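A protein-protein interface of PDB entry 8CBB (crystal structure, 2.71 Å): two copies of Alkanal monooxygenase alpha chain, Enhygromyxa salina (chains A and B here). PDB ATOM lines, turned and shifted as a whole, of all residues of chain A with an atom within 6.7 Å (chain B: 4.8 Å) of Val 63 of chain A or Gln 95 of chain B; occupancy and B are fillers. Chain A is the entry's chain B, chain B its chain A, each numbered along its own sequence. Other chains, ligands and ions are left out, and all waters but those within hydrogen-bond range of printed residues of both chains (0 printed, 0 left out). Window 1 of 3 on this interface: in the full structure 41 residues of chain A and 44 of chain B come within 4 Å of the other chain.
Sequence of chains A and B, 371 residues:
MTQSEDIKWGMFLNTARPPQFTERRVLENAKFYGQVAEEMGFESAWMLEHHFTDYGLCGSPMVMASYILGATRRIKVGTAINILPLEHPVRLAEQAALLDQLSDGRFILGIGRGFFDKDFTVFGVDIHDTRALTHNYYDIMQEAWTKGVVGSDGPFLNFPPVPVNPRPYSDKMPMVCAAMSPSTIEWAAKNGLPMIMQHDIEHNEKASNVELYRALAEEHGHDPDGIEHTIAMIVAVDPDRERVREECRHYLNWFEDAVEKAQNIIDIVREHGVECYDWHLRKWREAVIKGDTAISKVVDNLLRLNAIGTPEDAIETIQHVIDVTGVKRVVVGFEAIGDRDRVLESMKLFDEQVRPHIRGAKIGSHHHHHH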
ATOM      1  N   MET A  47      24.153  22.818   5.050  1.00  0.00           N
ATOM      2  CA  MET A  47      23.306  23.870   4.513  1.00  0.00           C
ATOM      3  C   MET A  47      22.242  24.243   5.542  1.00  0.00           C
ATOM      4  O   MET A  47      21.904  23.442   6.412  1.00  0.00           O
ATOM      5  CB  MET A  47      22.617  23.411   3.224  1.00  0.00           C
ATOM      6  CG  MET A  47      23.346  23.837   1.963  1.00  0.00           C
ATOM      7  SD  MET A  47      24.693  22.712   1.525  1.00  0.00           S
ATOM      8  CE  MET A  47      26.099  23.812   1.669  1.00  0.00           C
ATOM      9  N   CYS A  58      19.421  31.342   1.648  1.00  0.00           N
ATOM     10  CA  CYS A  58      18.983  30.019   1.237  1.00  0.00           C
ATOM     11  C   CYS A  58      17.715  29.640   1.996  1.00  0.00           C
ATOM     12  O   CYS A  58      17.712  29.592   3.223  1.00  0.00           O
ATOM     13  CB  CYS A  58      20.067  28.976   1.479  1.00  0.00           C
ATOM     14  SG  CYS A  58      19.531  27.286   1.102  1.00  0.00           S
ATOM     15  N   GLY A  59      16.642  29.376   1.243  1.00  0.00           N
ATOM     16  CA  GLY A  59      15.403  28.871   1.811  1.00  0.00           C
ATOM     17  C   GLY A  59      15.120  27.437   1.372  1.00  0.00           C
ATOM     18  O   GLY A  59      14.110  26.854   1.762  1.00  0.00           O
ATOM     19  N   SER A  60      16.028  26.881   0.560  1.00  0.00           N
ATOM     20  CA  SER A  60      15.932  25.499   0.118  1.00  0.00           C
ATOM     21  C   SER A  60      17.277  24.800   0.289  1.00  0.00           C
ATOM     22  O   SER A  60      18.086  24.761  -0.637  1.00  0.00           O
ATOM     23  CB  SER A  60      15.458  25.417  -1.310  1.00  0.00           C
ATOM     24  OG  SER A  60      15.286  24.064  -1.705  1.00  0.00           O
ATOM     25  N   PRO A  61      17.554  24.218   1.477  1.00  0.00           N
ATOM     26  CA  PRO A  61      18.767  23.428   1.684  1.00  0.00           C
ATOM     27  C   PRO A  61      18.841  22.203   0.776  1.00  0.00           C
ATOM     28  O   PRO A  61      19.931  21.752   0.434  1.00  0.00           O
ATOM     29  CB  PRO A  61      18.695  23.015   3.162  1.00  0.00           C
ATOM     30  CG  PRO A  61      17.227  23.143   3.525  1.00  0.00           C
ATOM     31  CD  PRO A  61      16.713  24.290   2.681  1.00  0.00           C
ATOM     32  N   MET A  62      17.675  21.676   0.386  1.00  0.00           N
ATOM     33  CA  MET A  62      17.606  20.506  -0.475  1.00  0.00           C
ATOM     34  C   MET A  62      18.188  20.845  -1.844  1.00  0.00           C
ATOM     35  O   MET A  62      18.908  20.044  -2.433  1.00  0.00           O
ATOM     36  CB  MET A  62      16.161  20.029  -0.653  1.00  0.00           C
ATOM     37  CG  MET A  62      15.693  19.081   0.435  1.00  0.00           C
ATOM     38  SD  MET A  62      16.902  17.787   0.801  1.00  0.00           S
ATOM     39  CE  MET A  62      16.099  16.359   0.070  1.00  0.00           C
ATOM     40  N   VAL A  63      17.857  22.041  -2.342  1.00  0.00           N
ATOM     41  CA  VAL A  63      18.307  22.480  -3.652  1.00  0.00           C
ATOM     42  C   VAL A  63      19.791  22.834  -3.575  1.00  0.00           C
ATOM     43  O   VAL A  63      20.562  22.496  -4.470  1.00  0.00           O
ATOM     44  CB  VAL A  63      17.471  23.668  -4.167  1.00  0.00           C
ATOM     45  CG1 VAL A  63      18.272  24.563  -5.100  1.00  0.00           C
ATOM     46  CG2 VAL A  63      16.189  23.199  -4.840  1.00  0.00           C
ATOM     47  N   MET A  64      20.179  23.526  -2.498  1.00  0.00           N
ATOM     48  CA  MET A  64      21.555  23.961  -2.340  1.00  0.00           C
ATOM     49  C   MET A  64      22.445  22.740  -2.129  1.00  0.00           C
ATOM     50  O   MET A  64      23.518  22.640  -2.720  1.00  0.00           O
ATOM     51  CB  MET A  64      21.706  24.920  -1.155  1.00  0.00           C
ATOM     52  CG  MET A  64      23.107  25.489  -1.023  1.00  0.00           C
ATOM     53  SD  MET A  64      23.154  27.056  -0.118  1.00  0.00           S
ATOM     54  CE  MET A  64      24.882  27.490  -0.314  1.00  0.00           C
ATOM     55  N   ALA A  65      21.978  21.812  -1.285  1.00  0.00           N
ATOM     56  CA  ALA A  65      22.710  20.590  -0.996  1.00  0.00           C
ATOM     57  C   ALA A  65      22.861  19.767  -2.271  1.00  0.00           C
ATOM     58  O   ALA A  65      23.909  19.173  -2.517  1.00  0.00           O
ATOM     59  CB  ALA A  65      21.998  19.805   0.078  1.00  0.00           C
ATOM     60  N   SER A  66      21.796  19.740  -3.078  1.00  0.00           N
ATOM     61  CA  SER A  66      21.772  18.942  -4.289  1.00  0.00           C
ATOM     62  C   SER A  66      22.790  19.489  -5.287  1.00  0.00           C
ATOM     63  O   SER A  66      23.412  18.728  -6.024  1.00  0.00           O
ATOM     64  CB  SER A  66      20.388  18.900  -4.875  1.00  0.00           C
ATOM     65  OG  SER A  66      20.353  18.057  -6.015  1.00  0.00           O
ATOM     66  N   TYR A  67      22.958  20.817  -5.291  1.00  0.00           N
ATOM     67  CA  TYR A  67      23.944  21.462  -6.141  1.00  0.00           C
ATOM     68  C   TYR A  67      25.349  21.058  -5.702  1.00  0.00           C
ATOM     69  O   TYR A  67      26.145  20.584  -6.510  1.00  0.00           O
ATOM     70  CB  TYR A  67      23.784  22.984  -6.110  1.00  0.00           C
ATOM     71  CG  TYR A  67      24.770  23.722  -6.979  1.00  0.00           C
ATOM     72  CD1 TYR A  67      24.511  23.948  -8.322  1.00  0.00           C
ATOM     73  CD2 TYR A  67      25.975  24.175  -6.468  1.00  0.00           C
ATOM     74  CE1 TYR A  67      25.417  24.615  -9.131  1.00  0.00           C
ATOM     75  CE2 TYR A  67      26.891  24.845  -7.264  1.00  0.00           C
ATOM     76  CZ  TYR A  67      26.612  25.065  -8.600  1.00  0.00           C
ATOM     77  OH  TYR A  67      27.514  25.727  -9.396  1.00  0.00           O
ATOM     78  N   ILE A  68      25.637  21.256  -4.410  1.00  0.00           N
ATOM     79  CA  ILE A  68      26.981  21.089  -3.881  1.00  0.00           C
ATOM     80  C   ILE A  68      27.427  19.646  -4.101  1.00  0.00           C
ATOM     81  O   ILE A  68      28.595  19.387  -4.380  1.00  0.00           O
ATOM     82  CB  ILE A  68      27.040  21.484  -2.391  1.00  0.00           C
ATOM     83  CG1 ILE A  68      26.658  22.951  -2.175  1.00  0.00           C
ATOM     84  CG2 ILE A  68      28.407  21.167  -1.803  1.00  0.00           C
ATOM     85  CD1 ILE A  68      27.622  23.937  -2.796  1.00  0.00           C
ATOM     86  N   GLU A  87       6.900  21.338   4.837  1.00  0.00           N
ATOM     87  CA  GLU A  87       6.974  20.480   3.665  1.00  0.00           C
ATOM     88  C   GLU A  87       5.975  19.337   3.816  1.00  0.00           C
ATOM     89  O   GLU A  87       5.792  18.811   4.911  1.00  0.00           O
ATOM     90  CB  GLU A  87       8.391  19.927   3.504  1.00  0.00           C
ATOM     91  CG  GLU A  87       9.273  20.763   2.594  1.00  0.00           C
ATOM     92  CD  GLU A  87       9.161  20.419   1.120  1.00  0.00           C
ATOM     93  OE1 GLU A  87      10.142  20.645   0.386  1.00  0.00           O
ATOM     94  OE2 GLU A  87       8.092  19.925   0.709  1.00  0.00           O
ATOM     95  N   GLN A  95      12.406  13.615  -2.405  1.00  0.00           N
ATOM     96  CA  GLN A  95      13.547  14.488  -2.628  1.00  0.00           C
ATOM     97  C   GLN A  95      14.807  13.832  -2.072  1.00  0.00           C
ATOM     98  O   GLN A  95      15.801  13.686  -2.781  1.00  0.00           O
ATOM     99  CB  GLN A  95      13.308  15.852  -1.977  1.00  0.00           C
ATOM    100  CG  GLN A  95      12.449  16.785  -2.819  1.00  0.00           C
ATOM    101  CD  GLN A  95      12.121  18.069  -2.098  1.00  0.00           C
ATOM    102  OE1 GLN A  95      12.735  18.416  -1.092  1.00  0.00           O
ATOM    103  NE2 GLN A  95      11.141  18.792  -2.615  1.00  0.00           N
ATOM    104  N   LEU A  99      18.169  12.200  -4.010  1.00  0.00           N
ATOM    105  CA  LEU A  99      19.468  12.827  -3.827  1.00  0.00           C
ATOM    106  C   LEU A  99      20.437  11.829  -3.198  1.00  0.00           C
ATOM    107  O   LEU A  99      21.642  11.904  -3.423  1.00  0.00           O
ATOM    108  CB  LEU A  99      19.308  14.069  -2.944  1.00  0.00           C
ATOM    109  CG  LEU A  99      20.597  14.839  -2.666  1.00  0.00           C
ATOM    110  CD1 LEU A  99      21.305  15.203  -3.964  1.00  0.00           C
ATOM    111  CD2 LEU A  99      20.320  16.086  -1.841  1.00  0.00           C
ATOM    112  N   MET B  62      13.550  19.816  -9.444  1.00  0.00           N
ATOM    113  CA  MET B  62      14.334  20.923  -8.922  1.00  0.00           C
ATOM    114  C   MET B  62      15.598  20.383  -8.260  1.00  0.00           C
ATOM    115  O   MET B  62      16.652  21.012  -8.319  1.00  0.00           O
ATOM    116  CB  MET B  62      13.536  21.738  -7.897  1.00  0.00           C
ATOM    117  CG  MET B  62      12.607  22.767  -8.523  1.00  0.00           C
ATOM    118  SD  MET B  62      13.457  23.950  -9.606  1.00  0.00           S
ATOM    119  CE  MET B  62      14.716  24.584  -8.499  1.00  0.00           C
ATOM    120  N   SER B  66      19.151  20.600  -9.970  1.00  0.00           N
ATOM    121  CA  SER B  66      20.149  21.248  -9.136  1.00  0.00           C
ATOM    122  C   SER B  66      21.444  20.438  -9.156  1.00  0.00           C
ATOM    123  O   SER B  66      22.532  21.005  -9.237  1.00  0.00           O
ATOM    124  CB  SER B  66      19.633  21.432  -7.731  1.00  0.00           C
ATOM    125  OG  SER B  66      20.193  22.592  -7.134  1.00  0.00           O
ATOM    126  N   GLU B  87       3.010  22.531  -5.413  1.00  0.00           N
ATOM    127  CA  GLU B  87       4.024  23.146  -4.572  1.00  0.00           C
ATOM    128  C   GLU B  87       3.637  24.594  -4.294  1.00  0.00           C
ATOM    129  O   GLU B  87       3.078  25.269  -5.156  1.00  0.00           O
ATOM    130  CB  GLU B  87       5.397  23.066  -5.243  1.00  0.00           C
ATOM    131  CG  GLU B  87       6.557  23.151  -4.266  1.00  0.00           C
ATOM    132  CD  GLU B  87       7.922  22.868  -4.873  1.00  0.00           C
ATOM    133  OE1 GLU B  87       7.995  22.685  -6.107  1.00  0.00           O
ATOM    134  OE2 GLU B  87       8.910  22.829  -4.110  1.00  0.00           O
ATOM    135  N   ARG B  91       7.796  28.846  -2.232  1.00  0.00           N
ATOM    136  CA  ARG B  91       8.854  27.884  -1.978  1.00  0.00           C
ATOM    137  C   ARG B  91       9.646  27.657  -3.263  1.00  0.00           C
ATOM    138  O   ARG B  91      10.872  27.583  -3.234  1.00  0.00           O
ATOM    139  CB  ARG B  91       8.264  26.577  -1.438  1.00  0.00           C
ATOM    140  CG  ARG B  91       9.304  25.534  -1.050  1.00  0.00           C
ATOM    141  CD  ARG B  91       9.095  24.979   0.348  1.00  0.00           C
ATOM    142  NE  ARG B  91       7.695  24.704   0.643  1.00  0.00           N
ATOM    143  CZ  ARG B  91       6.961  23.777   0.035  1.00  0.00           C
ATOM    144  NH1 ARG B  91       5.652  23.743   0.219  1.00  0.00           N
ATOM    145  NH2 ARG B  91       7.538  22.886  -0.754  1.00  0.00           N
ATOM    146  N   LEU B  92       8.930  27.559  -4.389  1.00  0.00           N
ATOM    147  CA  LEU B  92       9.553  27.296  -5.676  1.00  0.00           C
ATOM    148  C   LEU B  92      10.235  28.563  -6.186  1.00  0.00           C
ATOM    149  O   LEU B  92      11.243  28.492  -6.885  1.00  0.00           O
ATOM    150  CB  LEU B  92       8.486  26.807  -6.660  1.00  0.00           C
ATOM    151  CG  LEU B  92       8.980  26.520  -8.078  1.00  0.00           C
ATOM    152  CD1 LEU B  92      10.195  25.606  -8.058  1.00  0.00           C
ATOM    153  CD2 LEU B  92       7.872  25.912  -8.925  1.00  0.00           C
ATOM    154  N   ALA B  93       9.668  29.722  -5.834  1.00  0.00           N
ATOM    155  CA  ALA B  93      10.324  30.997  -6.065  1.00  0.00           C
ATOM    156  C   ALA B  93      11.718  30.972  -5.441  1.00  0.00           C
ATOM    157  O   ALA B  93      12.711  31.248  -6.112  1.00  0.00           O
ATOM    158  CB  ALA B  93       9.486  32.118  -5.501  1.00  0.00           C
ATOM    159  N   GLU B  94      11.771  30.632  -4.149  1.00  0.00           N
ATOM    160  CA  GLU B  94      13.029  30.523  -3.430  1.00  0.00           C
ATOM    161  C   GLU B  94      13.956  29.562  -4.170  1.00  0.00           C
ATOM    162  O   GLU B  94      15.147  29.830  -4.310  1.00  0.00           O
ATOM    163  CB  GLU B  94      12.778  30.061  -1.993  1.00  0.00           C
ATOM    164  CG  GLU B  94      12.360  31.184  -1.060  1.00  0.00           C
ATOM    165  CD  GLU B  94      11.864  30.734   0.303  1.00  0.00           C
ATOM    166  OE1 GLU B  94      11.666  31.606   1.177  1.00  0.00           O
ATOM    167  OE2 GLU B  94      11.671  29.515   0.490  1.00  0.00           O
ATOM    168  N   GLN B  95      13.393  28.443  -4.641  1.00  0.00           N
ATOM    169  CA  GLN B  95      14.179  27.352  -5.193  1.00  0.00           C
ATOM    170  C   GLN B  95      14.833  27.799  -6.498  1.00  0.00           C
ATOM    171  O   GLN B  95      16.024  27.579  -6.707  1.00  0.00           O
ATOM    172  CB  GLN B  95      13.299  26.120  -5.418  1.00  0.00           C
ATOM    173  CG  GLN B  95      12.989  25.353  -4.141  1.00  0.00           C
ATOM    174  CD  GLN B  95      12.227  24.075  -4.397  1.00  0.00           C
ATOM    175  OE1 GLN B  95      11.872  23.753  -5.529  1.00  0.00           O
ATOM    176  NE2 GLN B  95      11.967  23.331  -3.334  1.00  0.00           N
ATOM    177  N   ALA B  96      14.037  28.425  -7.372  1.00  0.00           N
ATOM    178  CA  ALA B  96      14.464  28.734  -8.726  1.00  0.00           C
ATOM    179  C   ALA B  96      15.449  29.900  -8.709  1.00  0.00           C
ATOM    180  O   ALA B  96      16.415  29.911  -9.468  1.00  0.00           O
ATOM    181  CB  ALA B  96      13.262  29.041  -9.585  1.00  0.00           C
ATOM    182  N   ALA B  97      15.189  30.880  -7.837  1.00  0.00           N
ATOM    183  CA  ALA B  97      16.031  32.061  -7.730  1.00  0.00           C
ATOM    184  C   ALA B  97      17.416  31.660  -7.230  1.00  0.00           C
ATOM    185  O   ALA B  97      18.427  32.155  -7.723  1.00  0.00           O
ATOM    186  CB  ALA B  97      15.385  33.072  -6.815  1.00  0.00           C
ATOM    187  N   LEU B  98      17.443  30.756  -6.246  1.00  0.00           N
ATOM    188  CA  LEU B  98      18.687  30.261  -5.682  1.00  0.00           C
ATOM    189  C   LEU B  98      19.472  29.525  -6.764  1.00  0.00           C
ATOM    190  O   LEU B  98      20.673  29.735  -6.914  1.00  0.00           O
ATOM    191  CB  LEU B  98      18.367  29.340  -4.499  1.00  0.00           C
ATOM    192  CG  LEU B  98      19.573  28.713  -3.799  1.00  0.00           C
ATOM    193  CD1 LEU B  98      20.518  29.780  -3.269  1.00  0.00           C
ATOM    194  CD2 LEU B  98      19.125  27.794  -2.670  1.00  0.00           C
ATOM    195  N   LEU B  99      18.774  28.666  -7.515  1.00  0.00           N
ATOM    196  CA  LEU B  99      19.414  27.802  -8.493  1.00  0.00           C
ATOM    197  C   LEU B  99      19.854  28.633  -9.694  1.00  0.00           C
ATOM    198  O   LEU B  99      20.799  28.272 -10.391  1.00  0.00           O
ATOM    199  CB  LEU B  99      18.434  26.700  -8.912  1.00  0.00           C
ATOM    200  CG  LEU B  99      19.028  25.591  -9.781  1.00  0.00           C
ATOM    201  CD1 LEU B  99      20.346  25.096  -9.205  1.00  0.00           C
ATOM    202  CD2 LEU B  99      18.049  24.437  -9.934  1.00  0.00           C
ATOM    203  N   LEU B 102      23.029  29.987  -8.132  1.00  0.00           N
ATOM    204  CA  LEU B 102      24.017  28.941  -7.929  1.00  0.00           C
ATOM    205  C   LEU B 102      24.581  28.504  -9.279  1.00  0.00           C
ATOM    206  O   LEU B 102      25.775  28.238  -9.397  1.00  0.00           O
ATOM    207  CB  LEU B 102      23.362  27.765  -7.198  1.00  0.00           C
ATOM    208  CG  LEU B 102      23.269  27.902  -5.679  1.00  0.00           C
ATOM    209  CD1 LEU B 102      22.861  26.582  -5.041  1.00  0.00           C
ATOM    210  CD2 LEU B 102      24.583  28.395  -5.093  1.00  0.00           C
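O of Val 63 of chain A lies within hydrogen-bond range of OG of Ser 66 of chain B, 2.7 Å away. The guanidinium group (NH2) of Arg 91 of chain B lies within salt-bridge range of the side-chain carboxylate (OE2) of Glu 87 of chain A. O of Leu 102 of chain B lies within hydrogen-bond range of OH of Tyr 67 of chain A.
Val 63 of chain A touches just these residues of chain B: Ser 66 (2.7 Å) and Gln 95 (3.9 Å). Of chain A, only Ser 60 and Val 63 come within 4 Å of Gln 95 of chain B. Of the printed residues of chain A, Arg 91 of chain B touches Glu 87 (3.3 Å). Of the printed residues of chain A, Leu 102 of chain B touches Met 64 (3.98 Å) and Tyr 67 (3.1 Å). Of the printed residues of chain A, Leu 98 of chain B touches Cys 58 (3.8 Å) and Ser 60 (3.8 Å). Of the printed residues of chain B, Met 64 of chain A touches Leu 102. Met 62 of chain A touches none of the printed residues of chain B.
Leu 98 of chain B touches Cys 58 of chain A (CD2 to SG, 3.8 Å). OE2 of Glu 94 of chain B touches O of Gly 59 of chain A (3.8 Å). Ser 60 of chain A touches Gln 95 of chain B (OG to CG, 3.6 Å). Ser 60 of chain A touches Leu 98 of chain B. Gln 95 of chain B touches Val 63 of chain A (CG to CG2, 3.9 Å). Leu 102 of chain B touches Met 64 of chain A. Ser 66 of chain A touches Ser 66 of chain B (OG to CB, 3.9 Å). Tyr 67 of chain A touches Ser 66 of chain B (CA to O, 3.4 Å).
Ser 66 of chain A touches its own counterpart, Ser 66 of chain B. Positions printed for both chains: 62, 66, 87, 95 and 99. Of the 11 pairs that touch across the chains among the printed residues, 1 has its exchanged pair printed and touching as well.
OE2 of Glu 87 of chain B is in salt-bridge range of NH2 of Arg 91 of chain B (3.6 Å). The side-chain carboxylate (OE2) of Glu 87 of chain B sits at hydrogen-bond distance from the side-chain amide nitrogen (NE2) of Gln 95 of chain B (3.2 Å). The backbone carbonyl oxygen of Ser 60 of chain A sits at hydrogen-bond distance from the side-chain sulfur of Cys 58 of chain A (3.4 Å). The side-chain hydroxyl of Ser 60 of chain A sits close to the backbone NH of Val 63 of chain A.
Among the printed residues, 11 pairs touch across the chains.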
